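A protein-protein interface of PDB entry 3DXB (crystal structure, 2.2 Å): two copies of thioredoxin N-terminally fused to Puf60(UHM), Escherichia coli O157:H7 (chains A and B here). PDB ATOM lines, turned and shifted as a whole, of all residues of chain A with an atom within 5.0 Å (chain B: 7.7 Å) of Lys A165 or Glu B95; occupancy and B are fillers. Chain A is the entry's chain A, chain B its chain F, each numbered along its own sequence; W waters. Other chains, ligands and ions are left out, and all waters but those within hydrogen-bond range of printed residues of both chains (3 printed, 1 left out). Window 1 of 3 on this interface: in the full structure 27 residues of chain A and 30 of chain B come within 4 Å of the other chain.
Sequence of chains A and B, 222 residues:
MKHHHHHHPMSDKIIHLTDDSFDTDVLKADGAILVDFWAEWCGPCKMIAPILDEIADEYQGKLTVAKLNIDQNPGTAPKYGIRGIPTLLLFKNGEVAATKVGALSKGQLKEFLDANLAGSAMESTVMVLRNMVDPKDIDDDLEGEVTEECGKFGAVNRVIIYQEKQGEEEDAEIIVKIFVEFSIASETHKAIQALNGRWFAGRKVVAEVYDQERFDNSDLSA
NE of Arg B130 lies within salt-bridge range of OE2 of Glu A168. The side-chain amino group (NZ) of Lys A165 lies within hydrogen-bond range of the backbone carbonyl oxygen (O) of Asn B93. OE1 of Glu A168 sits close to OE2 of Glu B208 (2.7 Å). N of Gly A167 sits at hydrogen-bond distance from OE2 of Glu B95, at 2.9 Å. NZ of Lys B92 lies within salt-bridge range of OE2 of Glu A168, at 3.2 Å. The side-chain carboxylate (OE1) of Glu A168 is in hydrogen-bond range of the side-chain amide nitrogen (ND2) of Asn B93 (2.6 Å). The backbone carbonyl oxygen (O) of Lys A165 lies close to the side-chain carboxylate (OE2) of Glu B95 (3.1 Å).
The side-chain carboxylate (OE2) of Glu B208 is in salt-bridge range of the side-chain amino group (NZ) of Lys B92 (3.3 Å). N of Gln A166 sits at hydrogen-bond distance from O of Glu A173 (2.8 Å). NZ of Lys A165 sits at hydrogen-bond distance from O of Glu A168 (3.4 Å). O of Leu B27 lies close to N of Gly B94 (3.5 Å). ND2 of Asn B93 is in hydrogen-bond range of OE2 of Glu B208 (3.3 Å). The backbone NH (N) of Arg B130 is in hydrogen-bond range of the backbone carbonyl oxygen (O) of Val B206 (2.7 Å).
Among the printed residues, pairs that only touch across the chains: Glu A168 with Glu B95, Lys A165 with Gly B94, Gln A166 with Glu B173, Glu A168 with Val B206, Gln A166 with Glu B95, Glu A169 with Val B206 and Gly A167 with Asn B93.
Lys A165 touches just these residues of chain B: Asn B93 (2.7 Å), Gly B94 (3.4 Å) and Glu B95 (3.1 Å). Printed residues of chain A within 4 Å of Glu B95: Lys A165 (3.1 Å), Gln A166 (3.8 Å), Gly A167 (2.9 Å) and Glu A168 (3.4 Å). Gly A167 touches just these residues of chain B: Asn B93 (3.9 Å) and Glu B95 (2.9 Å). Of the printed residues of chain B, Glu A168 touches Lys B92 (3.2 Å), Asn B93 (2.6 Å), Glu B95 (3.4 Å), Arg B130 (3.1 Å), Val B206 (3.7 Å) and Glu B208 (2.7 Å). Of the printed residues of chain A, Gly B94 touches Lys A165 (3.4 Å). Printed residues of chain B within 4 Å of Glu A169: Val B206. Printed residues of chain A within 4 Å of Arg B130: Glu A168 (3.1 Å). Printed residues of chain A within 4 Å of Lys B92: Glu A168. Lys B28 touches none of the printed residues of chain A. The nearest printed residue of chain A that does not touch Glu B95 is Ala A172 (6.2 Å).
Of the 21 printed residues of chain B, 8 touch a printed residue of chain A. Among the printed residues, 14 pairs touch across the chains. Among the printed residues, Asp or Glu carboxylates within 4 Å of a Lys or Arg side-chain nitrogen of the other chain: Glu A168 with Lys B92 (3.2 Å) and Glu A168 with Arg B130 (3.1 Å).
Gln A166 touches Glu B173, but with the chains exchanged Glu A173 does not touch Gln B166 (9.8 Å). Of the 14 pairs that touch across the chains among the printed residues, none has its exchanged pair printed and touching as well.
Water W1 bridges O of Leu B27 (2.5 Å) and NZ of Lys A165 (3.4 Å). Water W2 lies within hydrogen-bond range of OE2 of Glu A168 and OE1 of Glu B95. Water W3 bridges the backbone carbonyl oxygen (O) of Gly B94 and the backbone NH (N) of Lys A165.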
ATOM      1  N   GLN A 163     -23.202  -3.910  25.931  1.00  0.00           N
ATOM      2  CA  GLN A 163     -22.561  -2.612  25.790  1.00  0.00           C
ATOM      3  C   GLN A 163     -21.135  -2.804  25.289  1.00  0.00           C
ATOM      4  O   GLN A 163     -20.382  -3.613  25.836  1.00  0.00           O
ATOM      5  CB  GLN A 163     -22.585  -1.863  27.120  1.00  0.00           C
ATOM      6  CG  GLN A 163     -23.987  -1.640  27.671  1.00  0.00           C
ATOM      7  CD  GLN A 163     -23.984  -0.829  28.947  1.00  0.00           C
ATOM      8  OE1 GLN A 163     -23.529   0.314  28.966  1.00  0.00           O
ATOM      9  NE2 GLN A 163     -24.492  -1.415  30.023  1.00  0.00           N
ATOM     10  N   GLU A 164     -20.776  -2.075  24.235  1.00  0.00           N
ATOM     11  CA  GLU A 164     -19.472  -2.244  23.598  1.00  0.00           C
ATOM     12  C   GLU A 164     -18.712  -0.926  23.464  1.00  0.00           C
ATOM     13  O   GLU A 164     -19.193   0.021  22.841  1.00  0.00           O
ATOM     14  CB  GLU A 164     -19.633  -2.913  22.228  1.00  0.00           C
ATOM     15  CG  GLU A 164     -18.322  -3.321  21.569  1.00  0.00           C
ATOM     16  CD  GLU A 164     -18.529  -3.939  20.205  1.00  0.00           C
ATOM     17  OE1 GLU A 164     -18.892  -3.202  19.257  1.00  0.00           O
ATOM     18  OE2 GLU A 164     -18.319  -5.164  20.078  1.00  0.00           O
ATOM     19  N   LYS A 165     -17.519  -0.886  24.048  1.00  0.00           N
ATOM     20  CA  LYS A 165     -16.644   0.274  23.950  1.00  0.00           C
ATOM     21  C   LYS A 165     -16.002   0.318  22.564  1.00  0.00           C
ATOM     22  O   LYS A 165     -15.335  -0.632  22.148  1.00  0.00           O
ATOM     23  CB  LYS A 165     -15.581   0.230  25.046  1.00  0.00           C
ATOM     24  CG  LYS A 165     -14.863   1.544  25.283  1.00  0.00           C
ATOM     25  CD  LYS A 165     -13.802   1.388  26.354  1.00  0.00           C
ATOM     26  CE  LYS A 165     -12.897   2.599  26.396  1.00  0.00           C
ATOM     27  NZ  LYS A 165     -11.645   2.345  27.154  1.00  0.00           N
ATOM     28  N   GLN A 166     -16.212   1.432  21.864  1.00  0.00           N
ATOM     29  CA  GLN A 166     -15.816   1.581  20.459  1.00  0.00           C
ATOM     30  C   GLN A 166     -14.405   2.142  20.270  1.00  0.00           C
ATOM     31  O   GLN A 166     -14.127   2.851  19.298  1.00  0.00           O
ATOM     32  CB  GLN A 166     -16.834   2.455  19.714  1.00  0.00           C
ATOM     33  CG  GLN A 166     -18.251   1.886  19.685  1.00  0.00           C
ATOM     34  CD  GLN A 166     -18.325   0.534  19.005  1.00  0.00           C
ATOM     35  OE1 GLN A 166     -18.574  -0.479  19.651  1.00  0.00           O
ATOM     36  NE2 GLN A 166     -18.090   0.511  17.699  1.00  0.00           N
ATOM     37  N   GLY A 167     -13.513   1.804  21.193  1.00  0.00           N
ATOM     38  CA  GLY A 167     -12.145   2.292  21.154  1.00  0.00           C
ATOM     39  C   GLY A 167     -11.411   1.971  22.436  1.00  0.00           C
ATOM     40  O   GLY A 167     -12.013   1.527  23.417  1.00  0.00           O
ATOM     41  N   GLU A 168     -10.103   2.197  22.421  1.00  0.00           N
ATOM     42  CA  GLU A 168      -9.264   1.947  23.582  1.00  0.00           C
ATOM     43  C   GLU A 168      -9.044   3.213  24.404  1.00  0.00           C
ATOM     44  O   GLU A 168      -8.716   3.138  25.590  1.00  0.00           O
ATOM     45  CB  GLU A 168      -7.928   1.353  23.150  1.00  0.00           C
ATOM     46  CG  GLU A 168      -8.036  -0.056  22.593  1.00  0.00           C
ATOM     47  CD  GLU A 168      -6.683  -0.699  22.372  1.00  0.00           C
ATOM     48  OE1 GLU A 168      -5.769  -0.450  23.185  1.00  0.00           O
ATOM     49  OE2 GLU A 168      -6.534  -1.456  21.391  1.00  0.00           O
ATOM     50  N   GLU A 169      -9.225   4.371  23.768  1.00  0.00           N
ATOM     51  CA  GLU A 169      -9.132   5.662  24.455  1.00  0.00           C
ATOM     52  C   GLU A 169     -10.125   5.735  25.617  1.00  0.00           C
ATOM     53  O   GLU A 169     -11.236   5.215  25.520  1.00  0.00           O
ATOM     54  CB  GLU A 169      -9.315   6.836  23.477  1.00  0.00           C
ATOM     55  CG  GLU A 169     -10.706   6.990  22.849  1.00  0.00           C
ATOM     56  CD  GLU A 169     -10.913   6.160  21.585  1.00  0.00           C
ATOM     57  OE1 GLU A 169     -11.838   6.490  20.811  1.00  0.00           O
ATOM     58  OE2 GLU A 169     -10.168   5.183  21.358  1.00  0.00           O
ATOM     59  N   GLU A 170      -9.710   6.373  26.709  1.00  0.00           N
ATOM     60  CA  GLU A 170     -10.468   6.365  27.968  1.00  0.00           C
ATOM     61  C   GLU A 170     -11.956   6.694  27.847  1.00  0.00           C
ATOM     62  O   GLU A 170     -12.794   6.010  28.441  1.00  0.00           O
ATOM     63  CB  GLU A 170      -9.804   7.267  29.009  1.00  0.00           C
ATOM     64  CG  GLU A 170      -8.783   6.540  29.867  1.00  0.00           C
ATOM     65  CD  GLU A 170      -7.912   7.472  30.688  1.00  0.00           C
ATOM     66  OE1 GLU A 170      -8.319   8.632  30.936  1.00  0.00           O
ATOM     67  OE2 GLU A 170      -6.809   7.038  31.088  1.00  0.00           O
ATOM     68  N   ALA A 172     -13.857   6.634  25.012  1.00  0.00           N
ATOM     69  CA  ALA A 172     -14.423   6.095  23.781  1.00  0.00           C
ATOM     70  C   ALA A 172     -15.910   5.840  23.972  1.00  0.00           C
ATOM     71  O   ALA A 172     -16.344   5.437  25.056  1.00  0.00           O
ATOM     72  CB  ALA A 172     -13.717   4.812  23.387  1.00  0.00           C
ATOM     73  N   GLU A 173     -16.682   6.082  22.917  1.00  0.00           N
ATOM     74  CA  GLU A 173     -18.125   5.884  22.951  1.00  0.00           C
ATOM     75  C   GLU A 173     -18.480   4.423  23.208  1.00  0.00           C
ATOM     76  O   GLU A 173     -17.877   3.514  22.636  1.00  0.00           O
ATOM     77  CB  GLU A 173     -18.761   6.362  21.642  1.00  0.00           C
ATOM     78  CG  GLU A 173     -20.286   6.316  21.631  1.00  0.00           C
ATOM     79  CD  GLU A 173     -20.894   6.649  20.278  1.00  0.00           C
ATOM     80  OE1 GLU A 173     -20.142   6.940  19.322  1.00  0.00           O
ATOM     81  OE2 GLU A 173     -22.137   6.621  20.177  1.00  0.00           O
ATOM     82  N   ILE A 174     -19.451   4.212  24.091  1.00  0.00           N
ATOM     83  CA  ILE A 174     -20.031   2.895  24.303  1.00  0.00           C
ATOM     84  C   ILE A 174     -21.367   2.838  23.574  1.00  0.00           C
ATOM     85  O   ILE A 174     -22.203   3.728  23.739  1.00  0.00           O
ATOM     86  CB  ILE A 174     -20.230   2.593  25.806  1.00  0.00           C
ATOM     87  CG1 ILE A 174     -18.889   2.661  26.545  1.00  0.00           C
ATOM     88  CG2 ILE A 174     -20.891   1.226  26.002  1.00  0.00           C
ATOM     89  CD1 ILE A 174     -19.005   2.874  28.041  1.00  0.00           C
ATOM     90  N   VAL B  26     -12.029  -4.354  35.999  1.00  0.00           N
ATOM     91  CA  VAL B  26     -11.871  -4.919  34.661  1.00  0.00           C
ATOM     92  C   VAL B  26     -11.919  -3.847  33.572  1.00  0.00           C
ATOM     93  O   VAL B  26     -10.923  -3.615  32.882  1.00  0.00           O
ATOM     94  CB  VAL B  26     -12.934  -6.015  34.367  1.00  0.00           C
ATOM     95  CG1 VAL B  26     -12.642  -6.694  33.047  1.00  0.00           C
ATOM     96  CG2 VAL B  26     -12.984  -7.044  35.489  1.00  0.00           C
ATOM     97  N   LEU B  27     -13.075  -3.204  33.424  1.00  0.00           N
ATOM     98  CA  LEU B  27     -13.316  -2.279  32.314  1.00  0.00           C
ATOM     99  C   LEU B  27     -12.442  -1.026  32.355  1.00  0.00           C
ATOM    100  O   LEU B  27     -12.044  -0.508  31.312  1.00  0.00           O
ATOM    101  CB  LEU B  27     -14.799  -1.897  32.237  1.00  0.00           C
ATOM    102  CG  LEU B  27     -15.820  -3.016  31.992  1.00  0.00           C
ATOM    103  CD1 LEU B  27     -17.225  -2.443  31.839  1.00  0.00           C
ATOM    104  CD2 LEU B  27     -15.450  -3.850  30.775  1.00  0.00           C
ATOM    105  N   LYS B  28     -12.137  -0.555  33.559  1.00  0.00           N
ATOM    106  CA  LYS B  28     -11.352   0.667  33.724  1.00  0.00           C
ATOM    107  C   LYS B  28      -9.911   0.393  34.163  1.00  0.00           C
ATOM    108  O   LYS B  28      -9.177   1.315  34.524  1.00  0.00           O
ATOM    109  CB  LYS B  28     -12.056   1.623  34.694  1.00  0.00           C
ATOM    110  CG  LYS B  28     -13.378   2.162  34.165  1.00  0.00           C
ATOM    111  CD  LYS B  28     -13.889   3.307  35.012  1.00  0.00           C
ATOM    112  CE  LYS B  28     -15.054   4.016  34.337  1.00  0.00           C
ATOM    113  NZ  LYS B  28     -15.381   5.302  35.021  1.00  0.00           N
ATOM    114  N   ALA B  29      -9.510  -0.876  34.103  1.00  0.00           N
ATOM    115  CA  ALA B  29      -8.190  -1.302  34.567  1.00  0.00           C
ATOM    116  C   ALA B  29      -7.055  -0.941  33.613  1.00  0.00           C
ATOM    117  O   ALA B  29      -7.258  -0.820  32.401  1.00  0.00           O
ATOM    118  CB  ALA B  29      -8.185  -2.791  34.831  1.00  0.00           C
ATOM    119  N   ILE B  33      -6.672  -7.807  31.181  1.00  0.00           N
ATOM    120  CA  ILE B  33      -7.279  -8.578  32.265  1.00  0.00           C
ATOM    121  C   ILE B  33      -7.930  -9.837  31.706  1.00  0.00           C
ATOM    122  O   ILE B  33      -8.740  -9.763  30.782  1.00  0.00           O
ATOM    123  CB  ILE B  33      -8.351  -7.757  33.058  1.00  0.00           C
ATOM    124  CG1 ILE B  33      -7.924  -6.292  33.268  1.00  0.00           C
ATOM    125  CG2 ILE B  33      -8.714  -8.456  34.376  1.00  0.00           C
ATOM    126  CD1 ILE B  33      -6.719  -6.076  34.198  1.00  0.00           C
ATOM    127  N   TYR B  80     -22.515 -10.501  29.260  1.00  0.00           N
ATOM    128  CA  TYR B  80     -21.495 -10.871  28.283  1.00  0.00           C
ATOM    129  C   TYR B  80     -21.868 -12.130  27.497  1.00  0.00           C
ATOM    130  O   TYR B  80     -21.068 -12.650  26.714  1.00  0.00           O
ATOM    131  CB  TYR B  80     -20.132 -11.008  28.968  1.00  0.00           C
ATOM    132  CG  TYR B  80     -19.551  -9.673  29.381  1.00  0.00           C
ATOM    133  CD1 TYR B  80     -19.680  -9.206  30.688  1.00  0.00           C
ATOM    134  CD2 TYR B  80     -18.891  -8.865  28.455  1.00  0.00           C
ATOM    135  CE1 TYR B  80     -19.151  -7.972  31.065  1.00  0.00           C
ATOM    136  CE2 TYR B  80     -18.363  -7.636  28.817  1.00  0.00           C
ATOM    137  CZ  TYR B  80     -18.497  -7.195  30.120  1.00  0.00           C
ATOM    138  OH  TYR B  80     -17.970  -5.981  30.477  1.00  0.00           O
ATOM    139  N   LEU B  89     -12.734 -14.460  29.439  1.00  0.00           N
ATOM    140  CA  LEU B  89     -12.818 -13.272  28.593  1.00  0.00           C
ATOM    141  C   LEU B  89     -11.571 -12.416  28.758  1.00  0.00           C
ATOM    142  O   LEU B  89     -11.168 -12.102  29.883  1.00  0.00           O
ATOM    143  CB  LEU B  89     -14.069 -12.446  28.922  1.00  0.00           C
ATOM    144  CG  LEU B  89     -15.303 -12.568  28.020  1.00  0.00           C
ATOM    145  CD1 LEU B  89     -15.926 -13.947  28.095  1.00  0.00           C
ATOM    146  CD2 LEU B  89     -16.326 -11.507  28.385  1.00  0.00           C
ATOM    147  N   LEU B  90     -10.960 -12.046  27.635  1.00  0.00           N
ATOM    148  CA  LEU B  90      -9.786 -11.188  27.661  1.00  0.00           C
ATOM    149  C   LEU B  90     -10.176  -9.739  27.421  1.00  0.00           C
ATOM    150  O   LEU B  90     -10.708  -9.385  26.364  1.00  0.00           O
ATOM    151  CB  LEU B  90      -8.725 -11.646  26.650  1.00  0.00           C
ATOM    152  CG  LEU B  90      -7.353 -10.968  26.797  1.00  0.00           C
ATOM    153  CD1 LEU B  90      -6.638 -11.437  28.059  1.00  0.00           C
ATOM    154  CD2 LEU B  90      -6.474 -11.197  25.573  1.00  0.00           C
ATOM    155  N   PHE B  91      -9.907  -8.909  28.423  1.00  0.00           N
ATOM    156  CA  PHE B  91     -10.183  -7.485  28.355  1.00  0.00           C
ATOM    157  C   PHE B  91      -8.897  -6.701  28.177  1.00  0.00           C
ATOM    158  O   PHE B  91      -7.861  -7.043  28.755  1.00  0.00           O
ATOM    159  CB  PHE B  91     -10.895  -7.012  29.623  1.00  0.00           C
ATOM    160  CG  PHE B  91     -12.332  -7.437  29.709  1.00  0.00           C
ATOM    161  CD1 PHE B  91     -13.348  -6.605  29.241  1.00  0.00           C
ATOM    162  CD2 PHE B  91     -12.677  -8.667  30.267  1.00  0.00           C
ATOM    163  CE1 PHE B  91     -14.682  -6.996  29.325  1.00  0.00           C
ATOM    164  CE2 PHE B  91     -14.013  -9.062  30.358  1.00  0.00           C
ATOM    165  CZ  PHE B  91     -15.014  -8.225  29.883  1.00  0.00           C
ATOM    166  N   LYS B  92      -8.980  -5.655  27.364  1.00  0.00           N
ATOM    167  CA  LYS B  92      -7.906  -4.687  27.194  1.00  0.00           C
ATOM    168  C   LYS B  92      -8.531  -3.326  26.908  1.00  0.00           C
ATOM    169  O   LYS B  92      -9.266  -3.167  25.927  1.00  0.00           O
ATOM    170  CB  LYS B  92      -6.963  -5.096  26.055  1.00  0.00           C
ATOM    171  CG  LYS B  92      -5.830  -4.103  25.808  1.00  0.00           C
ATOM    172  CD  LYS B  92      -4.940  -4.484  24.611  1.00  0.00           C
ATOM    173  CE  LYS B  92      -5.576  -4.119  23.266  1.00  0.00           C
ATOM    174  NZ  LYS B  92      -4.548  -3.890  22.205  1.00  0.00           N
ATOM    175  N   ASN B  93      -8.244  -2.358  27.775  1.00  0.00           N
ATOM    176  CA  ASN B  93      -8.781  -0.998  27.658  1.00  0.00           C
ATOM    177  C   ASN B  93     -10.305  -0.941  27.474  1.00  0.00           C
ATOM    178  O   ASN B  93     -10.816  -0.165  26.666  1.00  0.00           O
ATOM    179  CB  ASN B  93      -8.049  -0.219  26.550  1.00  0.00           C
ATOM    180  CG  ASN B  93      -6.557  -0.060  26.827  1.00  0.00           C
ATOM    181  OD1 ASN B  93      -6.147   0.243  27.948  1.00  0.00           O
ATOM    182  ND2 ASN B  93      -5.739  -0.252  25.798  1.00  0.00           N
ATOM    183  N   GLY B  94     -11.020  -1.778  28.224  1.00  0.00           N
ATOM    184  CA  GLY B  94     -12.485  -1.787  28.204  1.00  0.00           C
ATOM    185  C   GLY B  94     -13.111  -2.466  26.999  1.00  0.00           C
ATOM    186  O   GLY B  94     -14.329  -2.431  26.821  1.00  0.00           O
ATOM    187  N   GLU B  95     -12.276  -3.085  26.170  1.00  0.00           N
ATOM    188  CA  GLU B  95     -12.743  -3.833  25.012  1.00  0.00           C
ATOM    189  C   GLU B  95     -12.545  -5.323  25.258  1.00  0.00           C
ATOM    190  O   GLU B  95     -11.570  -5.724  25.903  1.00  0.00           O
ATOM    191  CB  GLU B  95     -11.986  -3.399  23.757  1.00  0.00           C
ATOM    192  CG  GLU B  95     -12.197  -1.933  23.369  1.00  0.00           C
ATOM    193  CD  GLU B  95     -11.690  -1.607  21.974  1.00  0.00           C
ATOM    194  OE1 GLU B  95     -10.577  -2.045  21.611  1.00  0.00           O
ATOM    195  OE2 GLU B  95     -12.406  -0.905  21.233  1.00  0.00           O
ATOM    196  N   VAL B  96     -13.479  -6.136  24.765  1.00  0.00           N
ATOM    197  CA  VAL B  96     -13.323  -7.588  24.798  1.00  0.00           C
ATOM    198  C   VAL B  96     -12.430  -7.997  23.628  1.00  0.00           C
ATOM    199  O   VAL B  96     -12.832  -7.919  22.463  1.00  0.00           O
ATOM    200  CB  VAL B  96     -14.684  -8.339  24.766  1.00  0.00           C
ATOM    201  CG1 VAL B  96     -14.465  -9.844  24.783  1.00  0.00           C
ATOM    202  CG2 VAL B  96     -15.552  -7.929  25.950  1.00  0.00           C
ATOM    203  N   ALA B  97     -11.207  -8.402  23.955  1.00  0.00           N
ATOM    204  CA  ALA B  97     -10.195  -8.737  22.954  1.00  0.00           C
ATOM    205  C   ALA B  97     -10.361 -10.152  22.402  1.00  0.00           C
ATOM    206  O   ALA B  97     -10.114 -10.392  21.218  1.00  0.00           O
ATOM    207  CB  ALA B  97      -8.793  -8.549  23.532  1.00  0.00           C
ATOM    208  N   ALA B  98     -10.771 -11.079  23.267  1.00  0.00           N
ATOM    209  CA  ALA B  98     -10.931 -12.488  22.899  1.00  0.00           C
ATOM    210  C   ALA B  98     -11.782 -13.226  23.928  1.00  0.00           C
ATOM    211  O   ALA B  98     -11.972 -12.741  25.045  1.00  0.00           O
ATOM    212  CB  ALA B  98      -9.570 -13.155  22.763  1.00  0.00           C
ATOM    213  N   ARG B 130      -2.890   4.808  18.885  1.00  0.00           N
ATOM    214  CA  ARG B 130      -4.339   4.846  18.724  1.00  0.00           C
ATOM    215  C   ARG B 130      -4.904   6.147  19.280  1.00  0.00           C
ATOM    216  O   ARG B 130      -4.388   6.688  20.262  1.00  0.00           O
ATOM    217  CB  ARG B 130      -4.995   3.645  19.408  1.00  0.00           C
ATOM    218  CG  ARG B 130      -4.458   2.293  18.947  1.00  0.00           C
ATOM    219  CD  ARG B 130      -5.127   1.153  19.692  1.00  0.00           C
ATOM    220  NE  ARG B 130      -4.354  -0.087  19.606  1.00  0.00           N
ATOM    221  CZ  ARG B 130      -4.549  -1.050  18.708  1.00  0.00           C
ATOM    222  NH1 ARG B 130      -5.501  -0.942  17.790  1.00  0.00           N
ATOM    223  NH2 ARG B 130      -3.786  -2.131  18.731  1.00  0.00           N
ATOM    224  N   GLN B 166     -14.072   0.098  11.030  1.00  0.00           N
ATOM    225  CA  GLN B 166     -14.442  -0.580  12.271  1.00  0.00           C
ATOM    226  C   GLN B 166     -15.770  -1.320  12.125  1.00  0.00           C
ATOM    227  O   GLN B 166     -16.817  -0.836  12.565  1.00  0.00           O
ATOM    228  CB  GLN B 166     -14.508   0.413  13.438  1.00  0.00           C
ATOM    229  CG  GLN B 166     -13.210   1.157  13.713  1.00  0.00           C
ATOM    230  CD  GLN B 166     -12.132   0.270  14.308  1.00  0.00           C
ATOM    231  OE1 GLN B 166     -12.106   0.024  15.516  1.00  0.00           O
ATOM    232  NE2 GLN B 166     -11.227  -0.203  13.464  1.00  0.00           N
ATOM    233  N   GLU B 173     -17.622   3.374  11.186  1.00  0.00           N
ATOM    234  CA  GLU B 173     -16.646   4.424  11.435  1.00  0.00           C
ATOM    235  C   GLU B 173     -15.270   3.997  10.911  1.00  0.00           C
ATOM    236  O   GLU B 173     -14.878   2.828  11.018  1.00  0.00           O
ATOM    237  CB  GLU B 173     -16.603   4.749  12.943  1.00  0.00           C
ATOM    238  CG  GLU B 173     -15.326   4.300  13.683  1.00  0.00           C
ATOM    239  CD  GLU B 173     -15.600   3.652  15.042  1.00  0.00           C
ATOM    240  OE1 GLU B 173     -16.699   3.088  15.238  1.00  0.00           O
ATOM    241  OE2 GLU B 173     -14.700   3.689  15.911  1.00  0.00           O
ATOM    242  N   VAL B 206      -3.407   6.327  22.980  1.00  0.00           N
ATOM    243  CA  VAL B 206      -3.022   4.999  23.424  1.00  0.00           C
ATOM    244  C   VAL B 206      -1.816   4.558  22.590  1.00  0.00           C
ATOM    245  O   VAL B 206      -1.886   4.504  21.361  1.00  0.00           O
ATOM    246  CB  VAL B 206      -4.192   3.990  23.277  1.00  0.00           C
ATOM    247  CG1 VAL B 206      -3.796   2.620  23.782  1.00  0.00           C
ATOM    248  CG2 VAL B 206      -5.427   4.483  24.023  1.00  0.00           C
ATOM    249  N   GLU B 208       0.903   1.412  22.303  1.00  0.00           N
ATOM    250  CA  GLU B 208       1.075   0.011  22.697  1.00  0.00           C
ATOM    251  C   GLU B 208       2.019  -0.702  21.751  1.00  0.00           C
ATOM    252  O   GLU B 208       2.234  -0.248  20.627  1.00  0.00           O
ATOM    253  CB  GLU B 208      -0.261  -0.733  22.629  1.00  0.00           C
ATOM    254  CG  GLU B 208      -1.415  -0.077  23.337  1.00  0.00           C
ATOM    255  CD  GLU B 208      -2.729  -0.731  22.996  1.00  0.00           C
ATOM    256  OE1 GLU B 208      -3.165  -0.634  21.830  1.00  0.00           O
ATOM    257  OE2 GLU B 208      -3.328  -1.340  23.904  1.00  0.00           O
HETATM  258  O   HOH W   1     -13.065   1.317  30.018  1.00  0.00           O
HETATM  259  O   HOH W   2      -8.313  -2.118  19.527  1.00  0.00           O
HETATM  260  O   HOH W   3     -16.497  -3.329  25.259  1.00  0.00           O
